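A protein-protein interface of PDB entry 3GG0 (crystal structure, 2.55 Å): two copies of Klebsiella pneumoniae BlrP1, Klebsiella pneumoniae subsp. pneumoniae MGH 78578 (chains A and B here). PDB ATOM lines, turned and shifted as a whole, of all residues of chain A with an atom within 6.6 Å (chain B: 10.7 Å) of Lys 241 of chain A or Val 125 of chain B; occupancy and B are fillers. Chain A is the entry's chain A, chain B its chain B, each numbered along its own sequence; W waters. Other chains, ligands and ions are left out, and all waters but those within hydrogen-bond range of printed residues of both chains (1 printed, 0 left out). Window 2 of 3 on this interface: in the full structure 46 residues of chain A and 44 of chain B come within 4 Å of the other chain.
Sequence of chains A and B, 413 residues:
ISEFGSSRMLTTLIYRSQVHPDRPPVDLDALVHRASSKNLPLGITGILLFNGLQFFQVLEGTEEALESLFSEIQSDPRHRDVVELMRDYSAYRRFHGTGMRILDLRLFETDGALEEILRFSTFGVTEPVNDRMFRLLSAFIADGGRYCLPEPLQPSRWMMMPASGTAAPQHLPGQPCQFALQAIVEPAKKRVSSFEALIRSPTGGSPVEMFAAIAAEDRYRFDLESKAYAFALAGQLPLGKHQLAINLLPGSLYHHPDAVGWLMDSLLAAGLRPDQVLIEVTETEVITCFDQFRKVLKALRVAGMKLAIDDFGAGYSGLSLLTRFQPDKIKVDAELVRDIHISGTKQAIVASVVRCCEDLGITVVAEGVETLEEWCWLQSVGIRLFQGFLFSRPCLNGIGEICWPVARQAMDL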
ATOM      1  N   ARG A 191     -13.639  16.185 -13.701  1.00  0.00           N
ATOM      2  CA  ARG A 191     -15.086  16.176 -13.815  1.00  0.00           C
ATOM      3  C   ARG A 191     -15.607  17.511 -14.347  1.00  0.00           C
ATOM      4  O   ARG A 191     -15.169  18.572 -13.918  1.00  0.00           O
ATOM      5  CB  ARG A 191     -15.711  15.873 -12.445  1.00  0.00           C
ATOM      6  CG  ARG A 191     -17.232  15.909 -12.406  1.00  0.00           C
ATOM      7  CD  ARG A 191     -17.747  15.919 -10.959  1.00  0.00           C
ATOM      8  NE  ARG A 191     -17.523  17.208 -10.294  1.00  0.00           N
ATOM      9  CZ  ARG A 191     -18.493  18.022  -9.877  1.00  0.00           C
ATOM     10  NH1 ARG A 191     -19.767  17.684 -10.045  1.00  0.00           N
ATOM     11  NH2 ARG A 191     -18.189  19.173  -9.282  1.00  0.00           N
ATOM     12  N   SER A 193     -18.303  20.126 -14.112  1.00  0.00           N
ATOM     13  CA  SER A 193     -19.280  20.554 -13.122  1.00  0.00           C
ATOM     14  C   SER A 193     -20.550  21.039 -13.805  1.00  0.00           C
ATOM     15  O   SER A 193     -21.657  20.608 -13.467  1.00  0.00           O
ATOM     16  CB  SER A 193     -18.704  21.667 -12.249  1.00  0.00           C
ATOM     17  OG  SER A 193     -19.608  22.015 -11.216  1.00  0.00           O
ATOM     18  N   PRO A 238     -27.653  14.811 -23.885  1.00  0.00           N
ATOM     19  CA  PRO A 238     -28.824  15.268 -23.144  1.00  0.00           C
ATOM     20  C   PRO A 238     -28.503  15.740 -21.719  1.00  0.00           C
ATOM     21  O   PRO A 238     -29.357  15.630 -20.830  1.00  0.00           O
ATOM     22  CB  PRO A 238     -29.685  14.009 -23.082  1.00  0.00           C
ATOM     23  CG  PRO A 238     -28.658  12.842 -23.095  1.00  0.00           C
ATOM     24  CD  PRO A 238     -27.313  13.426 -23.521  1.00  0.00           C
ATOM     25  N   LEU A 239     -27.273  16.219 -21.506  1.00  0.00           N
ATOM     26  CA  LEU A 239     -26.876  16.927 -20.260  1.00  0.00           C
ATOM     27  C   LEU A 239     -26.790  16.041 -19.012  1.00  0.00           C
ATOM     28  O   LEU A 239     -25.762  16.012 -18.335  1.00  0.00           O
ATOM     29  CB  LEU A 239     -27.777  18.142 -19.994  1.00  0.00           C
ATOM     30  CG  LEU A 239     -27.381  19.037 -18.817  1.00  0.00           C
ATOM     31  CD1 LEU A 239     -26.039  19.715 -19.074  1.00  0.00           C
ATOM     32  CD2 LEU A 239     -28.461  20.069 -18.543  1.00  0.00           C
ATOM     33  N   GLY A 240     -27.886  15.363 -18.687  1.00  0.00           N
ATOM     34  CA  GLY A 240     -27.897  14.401 -17.597  1.00  0.00           C
ATOM     35  C   GLY A 240     -27.885  15.047 -16.227  1.00  0.00           C
ATOM     36  O   GLY A 240     -28.898  15.580 -15.775  1.00  0.00           O
ATOM     37  N   LYS A 241     -26.732  15.000 -15.566  1.00  0.00           N
ATOM     38  CA  LYS A 241     -26.636  15.406 -14.164  1.00  0.00           C
ATOM     39  C   LYS A 241     -25.795  16.676 -13.971  1.00  0.00           C
ATOM     40  O   LYS A 241     -25.534  17.089 -12.840  1.00  0.00           O
ATOM     41  CB  LYS A 241     -26.073  14.260 -13.314  1.00  0.00           C
ATOM     42  CG  LYS A 241     -26.806  12.929 -13.488  1.00  0.00           C
ATOM     43  CD  LYS A 241     -26.038  11.787 -12.820  1.00  0.00           C
ATOM     44  CE  LYS A 241     -26.294  10.452 -13.523  1.00  0.00           C
ATOM     45  NZ  LYS A 241     -27.648   9.904 -13.222  1.00  0.00           N
ATOM     46  N   HIS A 242     -25.379  17.288 -15.077  1.00  0.00           N
ATOM     47  CA  HIS A 242     -24.607  18.527 -15.028  1.00  0.00           C
ATOM     48  C   HIS A 242     -25.527  19.742 -14.983  1.00  0.00           C
ATOM     49  O   HIS A 242     -26.624  19.714 -15.532  1.00  0.00           O
ATOM     50  CB  HIS A 242     -23.680  18.622 -16.238  1.00  0.00           C
ATOM     51  CG  HIS A 242     -22.900  17.374 -16.497  1.00  0.00           C
ATOM     52  ND1 HIS A 242     -23.318  16.407 -17.384  1.00  0.00           N
ATOM     53  CD2 HIS A 242     -21.734  16.926 -15.975  1.00  0.00           C
ATOM     54  CE1 HIS A 242     -22.439  15.421 -17.404  1.00  0.00           C
ATOM     55  NE2 HIS A 242     -21.468  15.712 -16.558  1.00  0.00           N
ATOM     56  N   GLN A 243     -25.070  20.808 -14.328  1.00  0.00           N
ATOM     57  CA  GLN A 243     -25.819  22.063 -14.276  1.00  0.00           C
ATOM     58  C   GLN A 243     -25.732  22.811 -15.600  1.00  0.00           C
ATOM     59  O   GLN A 243     -24.774  22.653 -16.349  1.00  0.00           O
ATOM     60  CB  GLN A 243     -25.293  22.965 -13.158  1.00  0.00           C
ATOM     61  CG  GLN A 243     -25.589  22.493 -11.752  1.00  0.00           C
ATOM     62  CD  GLN A 243     -25.094  23.475 -10.698  1.00  0.00           C
ATOM     63  OE1 GLN A 243     -23.909  23.812 -10.653  1.00  0.00           O
ATOM     64  NE2 GLN A 243     -26.005  23.944  -9.849  1.00  0.00           N
ATOM     65  N   ARG A 273     -34.319  19.999 -15.103  1.00  0.00           N
ATOM     66  CA  ARG A 273     -34.799  20.250 -13.753  1.00  0.00           C
ATOM     67  C   ARG A 273     -34.456  21.683 -13.334  1.00  0.00           C
ATOM     68  O   ARG A 273     -33.513  22.272 -13.858  1.00  0.00           O
ATOM     69  CB  ARG A 273     -34.186  19.236 -12.777  1.00  0.00           C
ATOM     70  CG  ARG A 273     -34.407  17.768 -13.174  1.00  0.00           C
ATOM     71  CD  ARG A 273     -35.884  17.392 -13.144  1.00  0.00           C
ATOM     72  NE  ARG A 273     -36.544  17.881 -11.935  1.00  0.00           N
ATOM     73  CZ  ARG A 273     -37.829  18.213 -11.864  1.00  0.00           C
ATOM     74  NH1 ARG A 273     -38.608  18.106 -12.934  1.00  0.00           N
ATOM     75  NH2 ARG A 273     -38.334  18.657 -10.722  1.00  0.00           N
ATOM     76  N   PRO A 274     -35.240  22.261 -12.404  1.00  0.00           N
ATOM     77  CA  PRO A 274     -34.978  23.638 -11.978  1.00  0.00           C
ATOM     78  C   PRO A 274     -33.632  23.759 -11.263  1.00  0.00           C
ATOM     79  O   PRO A 274     -32.870  24.687 -11.528  1.00  0.00           O
ATOM     80  CB  PRO A 274     -36.124  23.930 -11.000  1.00  0.00           C
ATOM     81  CG  PRO A 274     -37.135  22.855 -11.241  1.00  0.00           C
ATOM     82  CD  PRO A 274     -36.389  21.673 -11.696  1.00  0.00           C
ATOM     83  N   ASP A 275     -33.338  22.800 -10.387  1.00  0.00           N
ATOM     84  CA  ASP A 275     -32.073  22.766  -9.642  1.00  0.00           C
ATOM     85  C   ASP A 275     -30.873  22.541 -10.561  1.00  0.00           C
ATOM     86  O   ASP A 275     -29.727  22.606 -10.130  1.00  0.00           O
ATOM     87  CB  ASP A 275     -32.122  21.679  -8.560  1.00  0.00           C
ATOM     88  CG  ASP A 275     -32.852  20.423  -9.024  1.00  0.00           C
ATOM     89  OD1 ASP A 275     -34.050  20.521  -9.389  1.00  0.00           O
ATOM     90  OD2 ASP A 275     -32.230  19.340  -9.024  1.00  0.00           O
ATOM     91  N   GLN A 276     -31.158  22.283 -11.827  1.00  0.00           N
ATOM     92  CA  GLN A 276     -30.139  22.002 -12.817  1.00  0.00           C
ATOM     93  C   GLN A 276     -29.815  23.274 -13.605  1.00  0.00           C
ATOM     94  O   GLN A 276     -28.808  23.347 -14.302  1.00  0.00           O
ATOM     95  CB  GLN A 276     -30.648  20.918 -13.761  1.00  0.00           C
ATOM     96  CG  GLN A 276     -29.587  20.144 -14.459  1.00  0.00           C
ATOM     97  CD  GLN A 276     -30.154  19.035 -15.298  1.00  0.00           C
ATOM     98  OE1 GLN A 276     -31.367  18.951 -15.505  1.00  0.00           O
ATOM     99  NE2 GLN A 276     -29.285  18.165 -15.789  1.00  0.00           N
ATOM    100  N   TYR B  92     -37.595  22.415  -2.162  1.00  0.00           N
ATOM    101  CA  TYR B  92     -37.853  21.032  -1.779  1.00  0.00           C
ATOM    102  C   TYR B  92     -37.153  20.725  -0.466  1.00  0.00           C
ATOM    103  O   TYR B  92     -36.123  21.322  -0.151  1.00  0.00           O
ATOM    104  CB  TYR B  92     -37.375  20.063  -2.877  1.00  0.00           C
ATOM    105  CG  TYR B  92     -35.870  20.040  -3.081  1.00  0.00           C
ATOM    106  CD1 TYR B  92     -35.241  20.983  -3.896  1.00  0.00           C
ATOM    107  CD2 TYR B  92     -35.080  19.066  -2.468  1.00  0.00           C
ATOM    108  CE1 TYR B  92     -33.862  20.968  -4.085  1.00  0.00           C
ATOM    109  CE2 TYR B  92     -33.701  19.039  -2.651  1.00  0.00           C
ATOM    110  CZ  TYR B  92     -33.097  19.993  -3.460  1.00  0.00           C
ATOM    111  OH  TYR B  92     -31.729  19.970  -3.643  1.00  0.00           O
ATOM    112  N   ARG B  94     -34.733  18.829   1.690  1.00  0.00           N
ATOM    113  CA  ARG B  94     -33.552  17.981   1.584  1.00  0.00           C
ATOM    114  C   ARG B  94     -33.663  16.814   2.554  1.00  0.00           C
ATOM    115  O   ARG B  94     -33.279  15.695   2.234  1.00  0.00           O
ATOM    116  CB  ARG B  94     -32.281  18.786   1.867  1.00  0.00           C
ATOM    117  CG  ARG B  94     -31.747  19.571   0.674  1.00  0.00           C
ATOM    118  CD  ARG B  94     -32.617  20.775   0.344  1.00  0.00           C
ATOM    119  NE  ARG B  94     -31.943  21.707  -0.557  1.00  0.00           N
ATOM    120  CZ  ARG B  94     -32.564  22.647  -1.266  1.00  0.00           C
ATOM    121  NH1 ARG B  94     -33.884  22.777  -1.195  1.00  0.00           N
ATOM    122  NH2 ARG B  94     -31.867  23.450  -2.059  1.00  0.00           N
ATOM    123  N   SER B 121     -30.961  12.021   2.771  1.00  0.00           N
ATOM    124  CA  SER B 121     -31.072  13.256   2.011  1.00  0.00           C
ATOM    125  C   SER B 121     -30.897  13.076   0.509  1.00  0.00           C
ATOM    126  O   SER B 121     -30.117  12.237   0.056  1.00  0.00           O
ATOM    127  CB  SER B 121     -30.060  14.274   2.524  1.00  0.00           C
ATOM    128  OG  SER B 121     -28.750  13.731   2.507  1.00  0.00           O
ATOM    129  N   THR B 122     -31.637  13.875  -0.254  1.00  0.00           N
ATOM    130  CA  THR B 122     -31.382  14.048  -1.678  1.00  0.00           C
ATOM    131  C   THR B 122     -31.080  15.507  -1.955  1.00  0.00           C
ATOM    132  O   THR B 122     -31.606  16.395  -1.284  1.00  0.00           O
ATOM    133  CB  THR B 122     -32.596  13.644  -2.528  1.00  0.00           C
ATOM    134  OG1 THR B 122     -33.714  14.479  -2.198  1.00  0.00           O
ATOM    135  CG2 THR B 122     -32.961  12.195  -2.287  1.00  0.00           C
ATOM    136  N   PHE B 123     -30.238  15.755  -2.949  1.00  0.00           N
ATOM    137  CA  PHE B 123     -29.903  17.117  -3.331  1.00  0.00           C
ATOM    138  C   PHE B 123     -30.122  17.343  -4.824  1.00  0.00           C
ATOM    139  O   PHE B 123     -29.232  17.836  -5.532  1.00  0.00           O
ATOM    140  CB  PHE B 123     -28.466  17.449  -2.928  1.00  0.00           C
ATOM    141  CG  PHE B 123     -28.243  17.463  -1.441  1.00  0.00           C
ATOM    142  CD1 PHE B 123     -28.426  18.629  -0.708  1.00  0.00           C
ATOM    143  CD2 PHE B 123     -27.866  16.308  -0.768  1.00  0.00           C
ATOM    144  CE1 PHE B 123     -28.227  18.644   0.666  1.00  0.00           C
ATOM    145  CE2 PHE B 123     -27.669  16.317   0.604  1.00  0.00           C
ATOM    146  CZ  PHE B 123     -27.849  17.486   1.321  1.00  0.00           C
ATOM    147  N   GLY B 124     -31.312  16.972  -5.297  1.00  0.00           N
ATOM    148  CA  GLY B 124     -31.684  17.147  -6.697  1.00  0.00           C
ATOM    149  C   GLY B 124     -31.024  16.144  -7.624  1.00  0.00           C
ATOM    150  O   GLY B 124     -30.497  15.125  -7.177  1.00  0.00           O
ATOM    151  N   VAL B 125     -31.053  16.438  -8.920  1.00  0.00           N
ATOM    152  CA  VAL B 125     -30.432  15.576  -9.927  1.00  0.00           C
ATOM    153  C   VAL B 125     -28.911  15.725  -9.945  1.00  0.00           C
ATOM    154  O   VAL B 125     -28.189  14.796 -10.323  1.00  0.00           O
ATOM    155  CB  VAL B 125     -30.988  15.860 -11.350  1.00  0.00           C
ATOM    156  CG1 VAL B 125     -32.352  15.208 -11.534  1.00  0.00           C
ATOM    157  CG2 VAL B 125     -31.055  17.362 -11.617  1.00  0.00           C
ATOM    158  N   THR B 126     -28.433  16.896  -9.535  1.00  0.00           N
ATOM    159  CA  THR B 126     -27.011  17.214  -9.595  1.00  0.00           C
ATOM    160  C   THR B 126     -26.277  16.729  -8.344  1.00  0.00           C
ATOM    161  O   THR B 126     -26.902  16.310  -7.363  1.00  0.00           O
ATOM    162  CB  THR B 126     -26.777  18.732  -9.782  1.00  0.00           C
ATOM    163  OG1 THR B 126     -27.363  19.448  -8.689  1.00  0.00           O
ATOM    164  CG2 THR B 126     -27.404  19.212 -11.084  1.00  0.00           C
ATOM    165  N   GLU B 127     -24.949  16.778  -8.392  1.00  0.00           N
ATOM    166  CA  GLU B 127     -24.121  16.385  -7.261  1.00  0.00           C
ATOM    167  C   GLU B 127     -24.478  17.210  -6.016  1.00  0.00           C
ATOM    168  O   GLU B 127     -24.650  18.429  -6.104  1.00  0.00           O
ATOM    169  CB  GLU B 127     -22.642  16.563  -7.609  1.00  0.00           C
ATOM    170  CG  GLU B 127     -21.703  15.610  -6.881  1.00  0.00           C
ATOM    171  CD  GLU B 127     -21.806  14.182  -7.389  1.00  0.00           C
ATOM    172  OE1 GLU B 127     -22.013  13.993  -8.608  1.00  0.00           O
ATOM    173  OE2 GLU B 127     -21.673  13.250  -6.568  1.00  0.00           O
ATOM    174  N   PRO B 128     -24.628  16.532  -4.858  1.00  0.00           N
ATOM    175  CA  PRO B 128     -24.908  17.168  -3.563  1.00  0.00           C
ATOM    176  C   PRO B 128     -24.016  18.371  -3.256  1.00  0.00           C
ATOM    177  O   PRO B 128     -24.466  19.324  -2.616  1.00  0.00           O
ATOM    178  CB  PRO B 128     -24.644  16.037  -2.548  1.00  0.00           C
ATOM    179  CG  PRO B 128     -24.087  14.878  -3.359  1.00  0.00           C
ATOM    180  CD  PRO B 128     -24.574  15.070  -4.737  1.00  0.00           C
ATOM    181  N   VAL B 129     -22.771  18.332  -3.727  1.00  0.00           N
ATOM    182  CA  VAL B 129     -21.812  19.411  -3.483  1.00  0.00           C
ATOM    183  C   VAL B 129     -22.225  20.737  -4.155  1.00  0.00           C
ATOM    184  O   VAL B 129     -21.679  21.796  -3.846  1.00  0.00           O
ATOM    185  CB  VAL B 129     -20.361  19.001  -3.908  1.00  0.00           C
ATOM    186  CG1 VAL B 129     -20.133  19.251  -5.402  1.00  0.00           C
ATOM    187  CG2 VAL B 129     -19.323  19.732  -3.063  1.00  0.00           C
ATOM    188  N   ASN B 130     -23.211  20.673  -5.047  1.00  0.00           N
ATOM    189  CA  ASN B 130     -23.745  21.882  -5.678  1.00  0.00           C
ATOM    190  C   ASN B 130     -24.827  22.574  -4.846  1.00  0.00           C
ATOM    191  O   ASN B 130     -25.348  23.613  -5.244  1.00  0.00           O
ATOM    192  CB  ASN B 130     -24.266  21.581  -7.085  1.00  0.00           C
ATOM    193  CG  ASN B 130     -23.162  21.179  -8.042  1.00  0.00           C
ATOM    194  OD1 ASN B 130     -22.053  21.712  -7.993  1.00  0.00           O
ATOM    195  ND2 ASN B 130     -23.463  20.234  -8.923  1.00  0.00           N
ATOM    196  N   ASP B 131     -25.133  22.013  -3.678  1.00  0.00           N
ATOM    197  CA  ASP B 131     -26.148  22.585  -2.793  1.00  0.00           C
ATOM    198  C   ASP B 131     -25.535  23.280  -1.567  1.00  0.00           C
ATOM    199  O   ASP B 131     -24.698  22.706  -0.866  1.00  0.00           O
ATOM    200  CB  ASP B 131     -27.141  21.510  -2.351  1.00  0.00           C
ATOM    201  CG  ASP B 131     -28.447  22.096  -1.848  1.00  0.00           C
ATOM    202  OD1 ASP B 131     -28.441  22.757  -0.784  1.00  0.00           O
ATOM    203  OD2 ASP B 131     -29.483  21.890  -2.517  1.00  0.00           O
HETATM  204  O   HOH W   1     -21.589  19.554 -10.876  1.00  0.00           O
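The backbone NH of Val 125 of chain B is in hydrogen-bond range of the side-chain carboxylate of Asp 275 of chain A.
The side-chain hydroxyl (OH) of Tyr 92 of chain B sits at hydrogen-bond distance from the backbone NH (N) of Gly 124 of chain B (3.4 Å). The side-chain amide oxygen of Gln 276 of chain A is in hydrogen-bond range of the backbone NH of Arg 273 of chain A (3.2 Å).
NH1 of Arg 191 of chain A touches CB of Glu 127 of chain B, 3.9 Å away. CB of Lys 241 of chain A touches O of Val 125 of chain B, at 3.7 Å. O of Lys 241 of chain A touches CG2 of Thr 126 of chain B, at 3.3 Å. Gln 243 of chain A touches Thr 126 of chain B. CG of Asn 130 of chain B touches OE1 of Gln 243 of chain A, at 3.8 Å. CG of Arg 273 of chain A touches CG1 of Val 125 of chain B, at 3.7 Å. CA of Gly 124 of chain B touches OD2 of Asp 275 of chain A, at 3.2 Å.
Of the printed residues of chain B, Arg 191 of chain A touches Glu 127. Leu 239 of chain A touches none of the printed residues of chain B. No residue of chain B comes within 4 Å of Gly 240 of chain A. Lys 241 of chain A touches two residues of chain B. His 242 of chain A touches none of the printed residues of chain B. Of the printed residues of chain B, Gln 243 of chain A touches Thr 126 (3.8 Å) and Asn 130 (3.8 Å). Of chain B, only Gly 124 (3.2 Å) and Val 125 (3.1 Å) come within 4 Å of Asp 275 of chain A. Of the printed residues of chain A, Gly 124 of chain B touches Asp 275. Val 125 of chain B touches just these residues of chain A: Lys 241, Arg 273 and Asp 275. Of the printed residues of chain A, Thr 126 of chain B touches Lys 241 and Gln 243. Printed residues of chain A within 4 Å of Glu 127 of chain B: Arg 191 (3.9 Å). The nearest residue of chain B that does not touch Lys 241 of chain A is Glu 127 of chain B (4.5 Å).
Printed residues of chain A that touch a printed residue of chain B: Arg 191, Lys 241, Gln 243, Arg 273 and Asp 275. Of the 13 printed residues of chain B, 5 touch a printed residue of chain A. Printed residues of chain B that touch a printed residue of chain A: Gly 124, Val 125, Thr 126, Glu 127 and Asn 130. Hydrophobic or aromatic side chains of chain B within 4 Å of the printed part of chain A: Val 125. Among the printed residues, 8 pairs touch across the chains. Among the printed residues, no Asp or Glu carboxylate lies within 4 Å of a Lys or Arg side-chain nitrogen of the other chain.
No position is printed for both chains.
Water W1 lies within hydrogen-bond range of the guanidinium group of Arg 191 of chain A (2.7 Å), the side-chain amide nitrogen of Asn 130 of chain B (2.8 Å) and the backbone carbonyl oxygen of Ser 193 of chain A (2.8 Å).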
